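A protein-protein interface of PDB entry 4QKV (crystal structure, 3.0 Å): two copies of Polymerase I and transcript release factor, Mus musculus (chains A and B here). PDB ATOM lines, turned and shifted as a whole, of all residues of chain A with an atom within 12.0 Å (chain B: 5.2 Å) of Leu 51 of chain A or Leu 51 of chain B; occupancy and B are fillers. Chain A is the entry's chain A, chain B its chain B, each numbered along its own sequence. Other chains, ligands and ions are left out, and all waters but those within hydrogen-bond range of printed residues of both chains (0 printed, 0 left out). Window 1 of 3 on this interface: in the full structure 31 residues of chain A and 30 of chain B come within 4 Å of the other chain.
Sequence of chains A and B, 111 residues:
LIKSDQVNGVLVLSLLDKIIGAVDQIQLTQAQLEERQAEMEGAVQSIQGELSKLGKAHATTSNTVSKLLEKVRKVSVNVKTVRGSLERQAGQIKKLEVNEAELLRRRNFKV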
ATOM      1  N   GLY A  42      -8.088 -13.127 -23.462  1.00  0.00           N
ATOM      2  CA  GLY A  42      -6.795 -12.508 -23.673  1.00  0.00           C
ATOM      3  C   GLY A  42      -6.885 -11.001 -23.584  1.00  0.00           C
ATOM      4  O   GLY A  42      -5.952 -10.323 -23.140  1.00  0.00           O
ATOM      5  N   ALA A  43      -8.024 -10.478 -24.026  1.00  0.00           N
ATOM      6  CA  ALA A  43      -8.330  -9.065 -23.876  1.00  0.00           C
ATOM      7  C   ALA A  43      -8.527  -8.757 -22.402  1.00  0.00           C
ATOM      8  O   ALA A  43      -7.864  -7.903 -21.844  1.00  0.00           O
ATOM      9  CB  ALA A  43      -9.576  -8.695 -24.676  1.00  0.00           C
ATOM     10  N   VAL A  44      -9.444  -9.487 -21.788  1.00  0.00           N
ATOM     11  CA  VAL A  44      -9.802  -9.318 -20.391  1.00  0.00           C
ATOM     12  C   VAL A  44      -8.603  -9.352 -19.437  1.00  0.00           C
ATOM     13  O   VAL A  44      -8.556  -8.588 -18.474  1.00  0.00           O
ATOM     14  CB  VAL A  44     -10.839 -10.398 -19.985  1.00  0.00           C
ATOM     15  CG1 VAL A  44     -10.754 -10.723 -18.505  1.00  0.00           C
ATOM     16  CG2 VAL A  44     -12.272  -9.951 -20.393  1.00  0.00           C
ATOM     17  N   GLN A  45      -7.631 -10.216 -19.703  1.00  0.00           N
ATOM     18  CA  GLN A  45      -6.497 -10.344 -18.796  1.00  0.00           C
ATOM     19  C   GLN A  45      -5.564  -9.145 -18.980  1.00  0.00           C
ATOM     20  O   GLN A  45      -4.998  -8.625 -18.015  1.00  0.00           O
ATOM     21  CB  GLN A  45      -5.757 -11.667 -19.026  1.00  0.00           C
ATOM     22  CG  GLN A  45      -4.709 -11.643 -20.140  1.00  0.00           C
ATOM     23  CD  GLN A  45      -4.123 -13.013 -20.427  1.00  0.00           C
ATOM     24  OE1 GLN A  45      -4.798 -14.037 -20.281  1.00  0.00           O
ATOM     25  NE2 GLN A  45      -2.846 -13.038 -20.811  1.00  0.00           N
ATOM     26  N   SER A  46      -5.432  -8.701 -20.228  1.00  0.00           N
ATOM     27  CA  SER A  46      -4.615  -7.542 -20.576  1.00  0.00           C
ATOM     28  C   SER A  46      -5.204  -6.260 -19.993  1.00  0.00           C
ATOM     29  O   SER A  46      -4.479  -5.336 -19.575  1.00  0.00           O
ATOM     30  CB  SER A  46      -4.485  -7.434 -22.098  1.00  0.00           C
ATOM     31  OG  SER A  46      -4.520  -6.079 -22.528  1.00  0.00           O
ATOM     32  N   ILE A  47      -6.529  -6.230 -19.976  1.00  0.00           N
ATOM     33  CA  ILE A  47      -7.287  -5.195 -19.326  1.00  0.00           C
ATOM     34  C   ILE A  47      -6.985  -5.232 -17.836  1.00  0.00           C
ATOM     35  O   ILE A  47      -6.587  -4.222 -17.241  1.00  0.00           O
ATOM     36  CB  ILE A  47      -8.778  -5.385 -19.607  1.00  0.00           C
ATOM     37  CG1 ILE A  47      -9.108  -4.766 -20.967  1.00  0.00           C
ATOM     38  CG2 ILE A  47      -9.633  -4.801 -18.494  1.00  0.00           C
ATOM     39  CD1 ILE A  47     -10.563  -4.855 -21.356  1.00  0.00           C
ATOM     40  N   GLN A  48      -7.139  -6.410 -17.246  1.00  0.00           N
ATOM     41  CA  GLN A  48      -6.806  -6.605 -15.846  1.00  0.00           C
ATOM     42  C   GLN A  48      -5.384  -6.127 -15.572  1.00  0.00           C
ATOM     43  O   GLN A  48      -5.121  -5.444 -14.585  1.00  0.00           O
ATOM     44  CB  GLN A  48      -6.964  -8.076 -15.448  1.00  0.00           C
ATOM     45  CG  GLN A  48      -8.063  -8.331 -14.402  1.00  0.00           C
ATOM     46  CD  GLN A  48      -7.932  -7.450 -13.139  1.00  0.00           C
ATOM     47  OE1 GLN A  48      -6.850  -6.953 -12.820  1.00  0.00           O
ATOM     48  NE2 GLN A  48      -9.045  -7.265 -12.421  1.00  0.00           N
ATOM     49  N   GLY A  49      -4.472  -6.466 -16.472  1.00  0.00           N
ATOM     50  CA  GLY A  49      -3.085  -6.088 -16.300  1.00  0.00           C
ATOM     51  C   GLY A  49      -2.898  -4.587 -16.320  1.00  0.00           C
ATOM     52  O   GLY A  49      -2.181  -4.030 -15.491  1.00  0.00           O
ATOM     53  N   GLU A  50      -3.554  -3.936 -17.275  1.00  0.00           N
ATOM     54  CA  GLU A  50      -3.470  -2.487 -17.438  1.00  0.00           C
ATOM     55  C   GLU A  50      -4.079  -1.789 -16.245  1.00  0.00           C
ATOM     56  O   GLU A  50      -3.520  -0.837 -15.724  1.00  0.00           O
ATOM     57  CB  GLU A  50      -4.188  -2.049 -18.712  1.00  0.00           C
ATOM     58  CG  GLU A  50      -4.059  -0.589 -19.023  1.00  0.00           C
ATOM     59  CD  GLU A  50      -4.895  -0.188 -20.221  1.00  0.00           C
ATOM     60  OE1 GLU A  50      -5.503  -1.086 -20.841  1.00  0.00           O
ATOM     61  OE2 GLU A  50      -4.952   1.021 -20.542  1.00  0.00           O
ATOM     62  N   LEU A  51      -5.230  -2.301 -15.819  1.00  0.00           N
ATOM     63  CA  LEU A  51      -5.981  -1.759 -14.694  1.00  0.00           C
ATOM     64  C   LEU A  51      -5.263  -1.812 -13.352  1.00  0.00           C
ATOM     65  O   LEU A  51      -5.166  -0.811 -12.669  1.00  0.00           O
ATOM     66  CB  LEU A  51      -7.303  -2.501 -14.562  1.00  0.00           C
ATOM     67  CG  LEU A  51      -8.182  -2.147 -13.364  1.00  0.00           C
ATOM     68  CD1 LEU A  51      -8.501  -0.648 -13.330  1.00  0.00           C
ATOM     69  CD2 LEU A  51      -9.466  -2.970 -13.428  1.00  0.00           C
ATOM     70  N   SER A  52      -4.786  -2.982 -12.949  1.00  0.00           N
ATOM     71  CA  SER A  52      -4.175  -3.098 -11.632  1.00  0.00           C
ATOM     72  C   SER A  52      -2.894  -2.272 -11.618  1.00  0.00           C
ATOM     73  O   SER A  52      -2.474  -1.752 -10.580  1.00  0.00           O
ATOM     74  CB  SER A  52      -3.892  -4.562 -11.279  1.00  0.00           C
ATOM     75  OG  SER A  52      -2.747  -5.033 -11.966  1.00  0.00           O
ATOM     76  N   LYS A  53      -2.289  -2.152 -12.797  1.00  0.00           N
ATOM     77  CA  LYS A  53      -1.086  -1.354 -12.976  1.00  0.00           C
ATOM     78  C   LYS A  53      -1.412   0.102 -12.677  1.00  0.00           C
ATOM     79  O   LYS A  53      -0.654   0.793 -11.995  1.00  0.00           O
ATOM     80  CB  LYS A  53      -0.538  -1.519 -14.401  1.00  0.00           C
ATOM     81  CG  LYS A  53       0.800  -0.850 -14.652  1.00  0.00           C
ATOM     82  CD  LYS A  53       1.587  -1.539 -15.741  1.00  0.00           C
ATOM     83  CE  LYS A  53       1.868  -2.993 -15.367  1.00  0.00           C
ATOM     84  NZ  LYS A  53       2.324  -3.834 -16.524  1.00  0.00           N
ATOM     85  N   LEU A  54      -2.562   0.544 -13.174  1.00  0.00           N
ATOM     86  CA  LEU A  54      -3.039   1.898 -12.954  1.00  0.00           C
ATOM     87  C   LEU A  54      -3.427   2.174 -11.485  1.00  0.00           C
ATOM     88  O   LEU A  54      -3.189   3.266 -10.976  1.00  0.00           O
ATOM     89  CB  LEU A  54      -4.223   2.186 -13.887  1.00  0.00           C
ATOM     90  CG  LEU A  54      -4.785   3.613 -13.966  1.00  0.00           C
ATOM     91  CD1 LEU A  54      -3.706   4.681 -13.695  1.00  0.00           C
ATOM     92  CD2 LEU A  54      -5.470   3.869 -15.337  1.00  0.00           C
ATOM     93  N   GLY A  55      -4.014   1.202 -10.803  1.00  0.00           N
ATOM     94  CA  GLY A  55      -4.355   1.377  -9.406  1.00  0.00           C
ATOM     95  C   GLY A  55      -3.099   1.584  -8.581  1.00  0.00           C
ATOM     96  O   GLY A  55      -3.084   2.376  -7.634  1.00  0.00           O
ATOM     97  N   LYS A  56      -2.041   0.862  -8.944  1.00  0.00           N
ATOM     98  CA  LYS A  56      -0.750   1.023  -8.286  1.00  0.00           C
ATOM     99  C   LYS A  56      -0.247   2.422  -8.557  1.00  0.00           C
ATOM    100  O   LYS A  56       0.290   3.075  -7.662  1.00  0.00           O
ATOM    101  CB  LYS A  56       0.270  -0.023  -8.760  1.00  0.00           C
ATOM    102  CG  LYS A  56       0.022  -1.427  -8.230  1.00  0.00           C
ATOM    103  CD  LYS A  56       0.928  -2.435  -8.916  1.00  0.00           C
ATOM    104  CE  LYS A  56       0.337  -3.833  -8.866  1.00  0.00           C
ATOM    105  NZ  LYS A  56       0.452  -4.453 -10.214  1.00  0.00           N
ATOM    106  N   ALA A  57      -0.443   2.881  -9.791  1.00  0.00           N
ATOM    107  CA  ALA A  57      -0.087   4.247 -10.162  1.00  0.00           C
ATOM    108  C   ALA A  57      -0.775   5.250  -9.239  1.00  0.00           C
ATOM    109  O   ALA A  57      -0.110   6.112  -8.657  1.00  0.00           O
ATOM    110  CB  ALA A  57      -0.441   4.531 -11.616  1.00  0.00           C
ATOM    111  N   HIS A  58      -2.091   5.115  -9.082  1.00  0.00           N
ATOM    112  CA  HIS A  58      -2.864   6.051  -8.266  1.00  0.00           C
ATOM    113  C   HIS A  58      -2.540   6.012  -6.764  1.00  0.00           C
ATOM    114  O   HIS A  58      -2.638   7.032  -6.079  1.00  0.00           O
ATOM    115  CB  HIS A  58      -4.357   5.807  -8.442  1.00  0.00           C
ATOM    116  CG  HIS A  58      -5.214   6.777  -7.682  1.00  0.00           C
ATOM    117  ND1 HIS A  58      -5.869   6.434  -6.521  1.00  0.00           N
ATOM    118  CD2 HIS A  58      -5.513   8.075  -7.923  1.00  0.00           C
ATOM    119  CE1 HIS A  58      -6.549   7.484  -6.078  1.00  0.00           C
ATOM    120  NE2 HIS A  58      -6.350   8.488  -6.911  1.00  0.00           N
ATOM    121  N   ALA A  59      -2.190   4.838  -6.250  1.00  0.00           N
ATOM    122  CA  ALA A  59      -1.806   4.716  -4.856  1.00  0.00           C
ATOM    123  C   ALA A  59      -0.633   5.641  -4.587  1.00  0.00           C
ATOM    124  O   ALA A  59      -0.653   6.465  -3.668  1.00  0.00           O
ATOM    125  CB  ALA A  59      -1.440   3.281  -4.532  1.00  0.00           C
ATOM    126  N   THR A  60       0.390   5.489  -5.421  1.00  0.00           N
ATOM    127  CA  THR A  60       1.587   6.305  -5.347  1.00  0.00           C
ATOM    128  C   THR A  60       1.215   7.778  -5.304  1.00  0.00           C
ATOM    129  O   THR A  60       1.792   8.544  -4.541  1.00  0.00           O
ATOM    130  CB  THR A  60       2.525   6.044  -6.552  1.00  0.00           C
ATOM    131  OG1 THR A  60       3.009   4.691  -6.513  1.00  0.00           O
ATOM    132  CG2 THR A  60       3.707   7.021  -6.539  1.00  0.00           C
ATOM    133  N   SER B  46     -16.123  -0.730 -24.071  1.00  0.00           N
ATOM    134  CA  SER B  46     -16.390   0.394 -23.186  1.00  0.00           C
ATOM    135  C   SER B  46     -15.253   0.531 -22.191  1.00  0.00           C
ATOM    136  O   SER B  46     -14.535   1.517 -22.216  1.00  0.00           O
ATOM    137  CB  SER B  46     -17.710   0.199 -22.450  1.00  0.00           C
ATOM    138  OG  SER B  46     -18.789   0.111 -23.366  1.00  0.00           O
ATOM    139  N   ILE B  47     -15.094  -0.483 -21.344  1.00  0.00           N
ATOM    140  CA  ILE B  47     -14.035  -0.568 -20.331  1.00  0.00           C
ATOM    141  C   ILE B  47     -12.637  -0.179 -20.818  1.00  0.00           C
ATOM    142  O   ILE B  47     -11.919   0.526 -20.121  1.00  0.00           O
ATOM    143  CB  ILE B  47     -13.968  -1.998 -19.741  1.00  0.00           C
ATOM    144  CG1 ILE B  47     -15.237  -2.283 -18.936  1.00  0.00           C
ATOM    145  CG2 ILE B  47     -12.708  -2.215 -18.906  1.00  0.00           C
ATOM    146  CD1 ILE B  47     -15.374  -3.685 -18.436  1.00  0.00           C
ATOM    147  N   GLN B  48     -12.245  -0.600 -22.008  1.00  0.00           N
ATOM    148  CA  GLN B  48     -10.921  -0.235 -22.492  1.00  0.00           C
ATOM    149  C   GLN B  48     -10.901   1.254 -22.757  1.00  0.00           C
ATOM    150  O   GLN B  48      -9.918   1.936 -22.459  1.00  0.00           O
ATOM    151  CB  GLN B  48     -10.542  -1.010 -23.757  1.00  0.00           C
ATOM    152  CG  GLN B  48      -9.221  -0.577 -24.385  1.00  0.00           C
ATOM    153  CD  GLN B  48      -8.045  -0.727 -23.440  1.00  0.00           C
ATOM    154  OE1 GLN B  48      -7.511  -1.825 -23.269  1.00  0.00           O
ATOM    155  NE2 GLN B  48      -7.628   0.384 -22.819  1.00  0.00           N
ATOM    156  N   GLY B  49     -12.004   1.759 -23.301  1.00  0.00           N
ATOM    157  CA  GLY B  49     -12.101   3.169 -23.629  1.00  0.00           C
ATOM    158  C   GLY B  49     -11.979   4.004 -22.376  1.00  0.00           C
ATOM    159  O   GLY B  49     -11.283   5.020 -22.345  1.00  0.00           O
ATOM    160  N   GLU B  50     -12.646   3.552 -21.321  1.00  0.00           N
ATOM    161  CA  GLU B  50     -12.729   4.322 -20.094  1.00  0.00           C
ATOM    162  C   GLU B  50     -11.425   4.194 -19.329  1.00  0.00           C
ATOM    163  O   GLU B  50     -10.904   5.163 -18.756  1.00  0.00           O
ATOM    164  CB  GLU B  50     -13.923   3.861 -19.255  1.00  0.00           C
ATOM    165  CG  GLU B  50     -13.711   3.871 -17.748  1.00  0.00           C
ATOM    166  CD  GLU B  50     -15.029   3.758 -16.970  1.00  0.00           C
ATOM    167  OE1 GLU B  50     -15.987   3.127 -17.479  1.00  0.00           O
ATOM    168  OE2 GLU B  50     -15.112   4.312 -15.849  1.00  0.00           O
ATOM    169  N   LEU B  51     -10.873   2.994 -19.355  1.00  0.00           N
ATOM    170  CA  LEU B  51      -9.586   2.776 -18.737  1.00  0.00           C
ATOM    171  C   LEU B  51      -8.531   3.632 -19.457  1.00  0.00           C
ATOM    172  O   LEU B  51      -7.586   4.125 -18.847  1.00  0.00           O
ATOM    173  CB  LEU B  51      -9.243   1.284 -18.770  1.00  0.00           C
ATOM    174  CG  LEU B  51      -7.948   0.768 -18.165  1.00  0.00           C
ATOM    175  CD1 LEU B  51      -7.836   1.171 -16.707  1.00  0.00           C
ATOM    176  CD2 LEU B  51      -7.875  -0.760 -18.323  1.00  0.00           C
ATOM    177  N   SER B  52      -8.709   3.813 -20.760  1.00  0.00           N
ATOM    178  CA  SER B  52      -7.748   4.566 -21.543  1.00  0.00           C
ATOM    179  C   SER B  52      -7.817   6.030 -21.135  1.00  0.00           C
ATOM    180  O   SER B  52      -6.798   6.730 -21.131  1.00  0.00           O
ATOM    181  CB  SER B  52      -8.024   4.388 -23.042  1.00  0.00           C
ATOM    182  OG  SER B  52      -7.392   5.387 -23.835  1.00  0.00           O
ATOM    183  N   LYS B  53      -9.028   6.474 -20.789  1.00  0.00           N
ATOM    184  CA  LYS B  53      -9.293   7.849 -20.366  1.00  0.00           C
ATOM    185  C   LYS B  53      -8.773   8.113 -18.964  1.00  0.00           C
ATOM    186  O   LYS B  53      -8.065   9.091 -18.729  1.00  0.00           O
ATOM    187  CB  LYS B  53     -10.792   8.148 -20.408  1.00  0.00           C
ATOM    188  CG  LYS B  53     -11.254   8.801 -21.680  1.00  0.00           C
ATOM    189  CD  LYS B  53     -12.774   8.936 -21.769  1.00  0.00           C
ATOM    190  CE  LYS B  53     -13.150   9.545 -23.128  1.00  0.00           C
ATOM    191  NZ  LYS B  53     -14.609   9.535 -23.395  1.00  0.00           N
ATOM    192  N   LEU B  54      -9.128   7.242 -18.027  1.00  0.00           N
ATOM    193  CA  LEU B  54      -8.672   7.399 -16.649  1.00  0.00           C
ATOM    194  C   LEU B  54      -7.156   7.445 -16.573  1.00  0.00           C
ATOM    195  O   LEU B  54      -6.598   8.001 -15.653  1.00  0.00           O
ATOM    196  CB  LEU B  54      -9.197   6.262 -15.776  1.00  0.00           C
ATOM    197  CG  LEU B  54      -9.088   6.444 -14.269  1.00  0.00           C
ATOM    198  CD1 LEU B  54      -9.613   7.805 -13.888  1.00  0.00           C
ATOM    199  CD2 LEU B  54      -9.863   5.357 -13.534  1.00  0.00           C
ATOM    200  N   GLY B  55      -6.491   6.855 -17.551  1.00  0.00           N
ATOM    201  CA  GLY B  55      -5.050   6.813 -17.553  1.00  0.00           C
ATOM    202  C   GLY B  55      -4.465   8.146 -17.957  1.00  0.00           C
ATOM    203  O   GLY B  55      -3.443   8.557 -17.398  1.00  0.00           O
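Leu 51 of chain A touches just one residue of chain B: Leu 51.
Of chain A, only Ile 47 (3.8 Å), Glu 50 (3.5 Å), Leu 51 (3.9 Å) and Leu 54 (3.8 Å) come within 4 Å of Leu 51 of chain B.
No residue of chain A comes within 4 Å of Ile 47 of chain B.
No residue of chain A comes within 4 Å of Gly 49 of chain B.
No residue of chain A comes within 4 Å of Leu 54 of chain B.
Of the printed residues of chain A, Gly 55 of chain B touches Leu 54.
Of the printed residues of chain B, Leu 54 of chain A touches Leu 51 (3.8 Å) and Gly 55 (3.7 Å).
Printed residues of chain B within 4 Å of Ile 47 of chain A: Leu 51.
Printed residues of chain B within 4 Å of Glu 50 of chain A: Gln 48 (3.2 Å) and Leu 51 (3.5 Å).
Gln 48 of chain A touches none of the printed residues of chain B.
Ala 59 of chain A touches none of the printed residues of chain B.
Among the printed residues, merely in contact across the chains: Glu 50 of chain A with Leu 51 of chain B, Leu 54 of chain A with Gly 55 of chain B, Leu 54 of chain A with Leu 51 of chain B, Ile 47 of chain A with Leu 51 of chain B and Leu 51 of chain A with Leu 51 of chain B.
Ile 47 of chain A touches Leu 51 of chain B, but with the chains exchanged Leu 51 of chain A does not touch Ile 47 of chain B (6.4 Å).
Glu 50 of chain A touches Gln 48 of chain B, but with the chains exchanged Gln 48 of chain A does not touch Glu 50 of chain B (11.6 Å).
Glu 50 of chain A touches Leu 51 of chain B, but with the chains exchanged Leu 51 of chain A does not touch Glu 50 of chain B (8.2 Å).
Leu 54 of chain A touches Leu 51 of chain B, but with the chains exchanged Leu 51 of chain A does not touch Leu 54 of chain B (6.2 Å).
Of the 6 pairs that touch across the chains among the printed residues, 1 has its exchanged pair printed and touching as well.
Of the 10 printed residues of chain B, 3 touch a printed residue of chain A.
Printed residues of chain B that touch a printed residue of chain A: Gln 48, Leu 51 and Gly 55.
Hydrophobic or aromatic side chains of chain B that line the printed part of chain A: Leu 51.
Hydrophobic or aromatic side chains of chain A within 4 Å of the printed part of chain B: Leu 51 and Leu 54.
Among the printed residues, 6 pairs touch across the chains.
The side-chain carboxylate (OE1) of Glu 50 of chain A sits close to the side-chain amide oxygen (OE1) of Gln 48 of chain B (3.2 Å).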
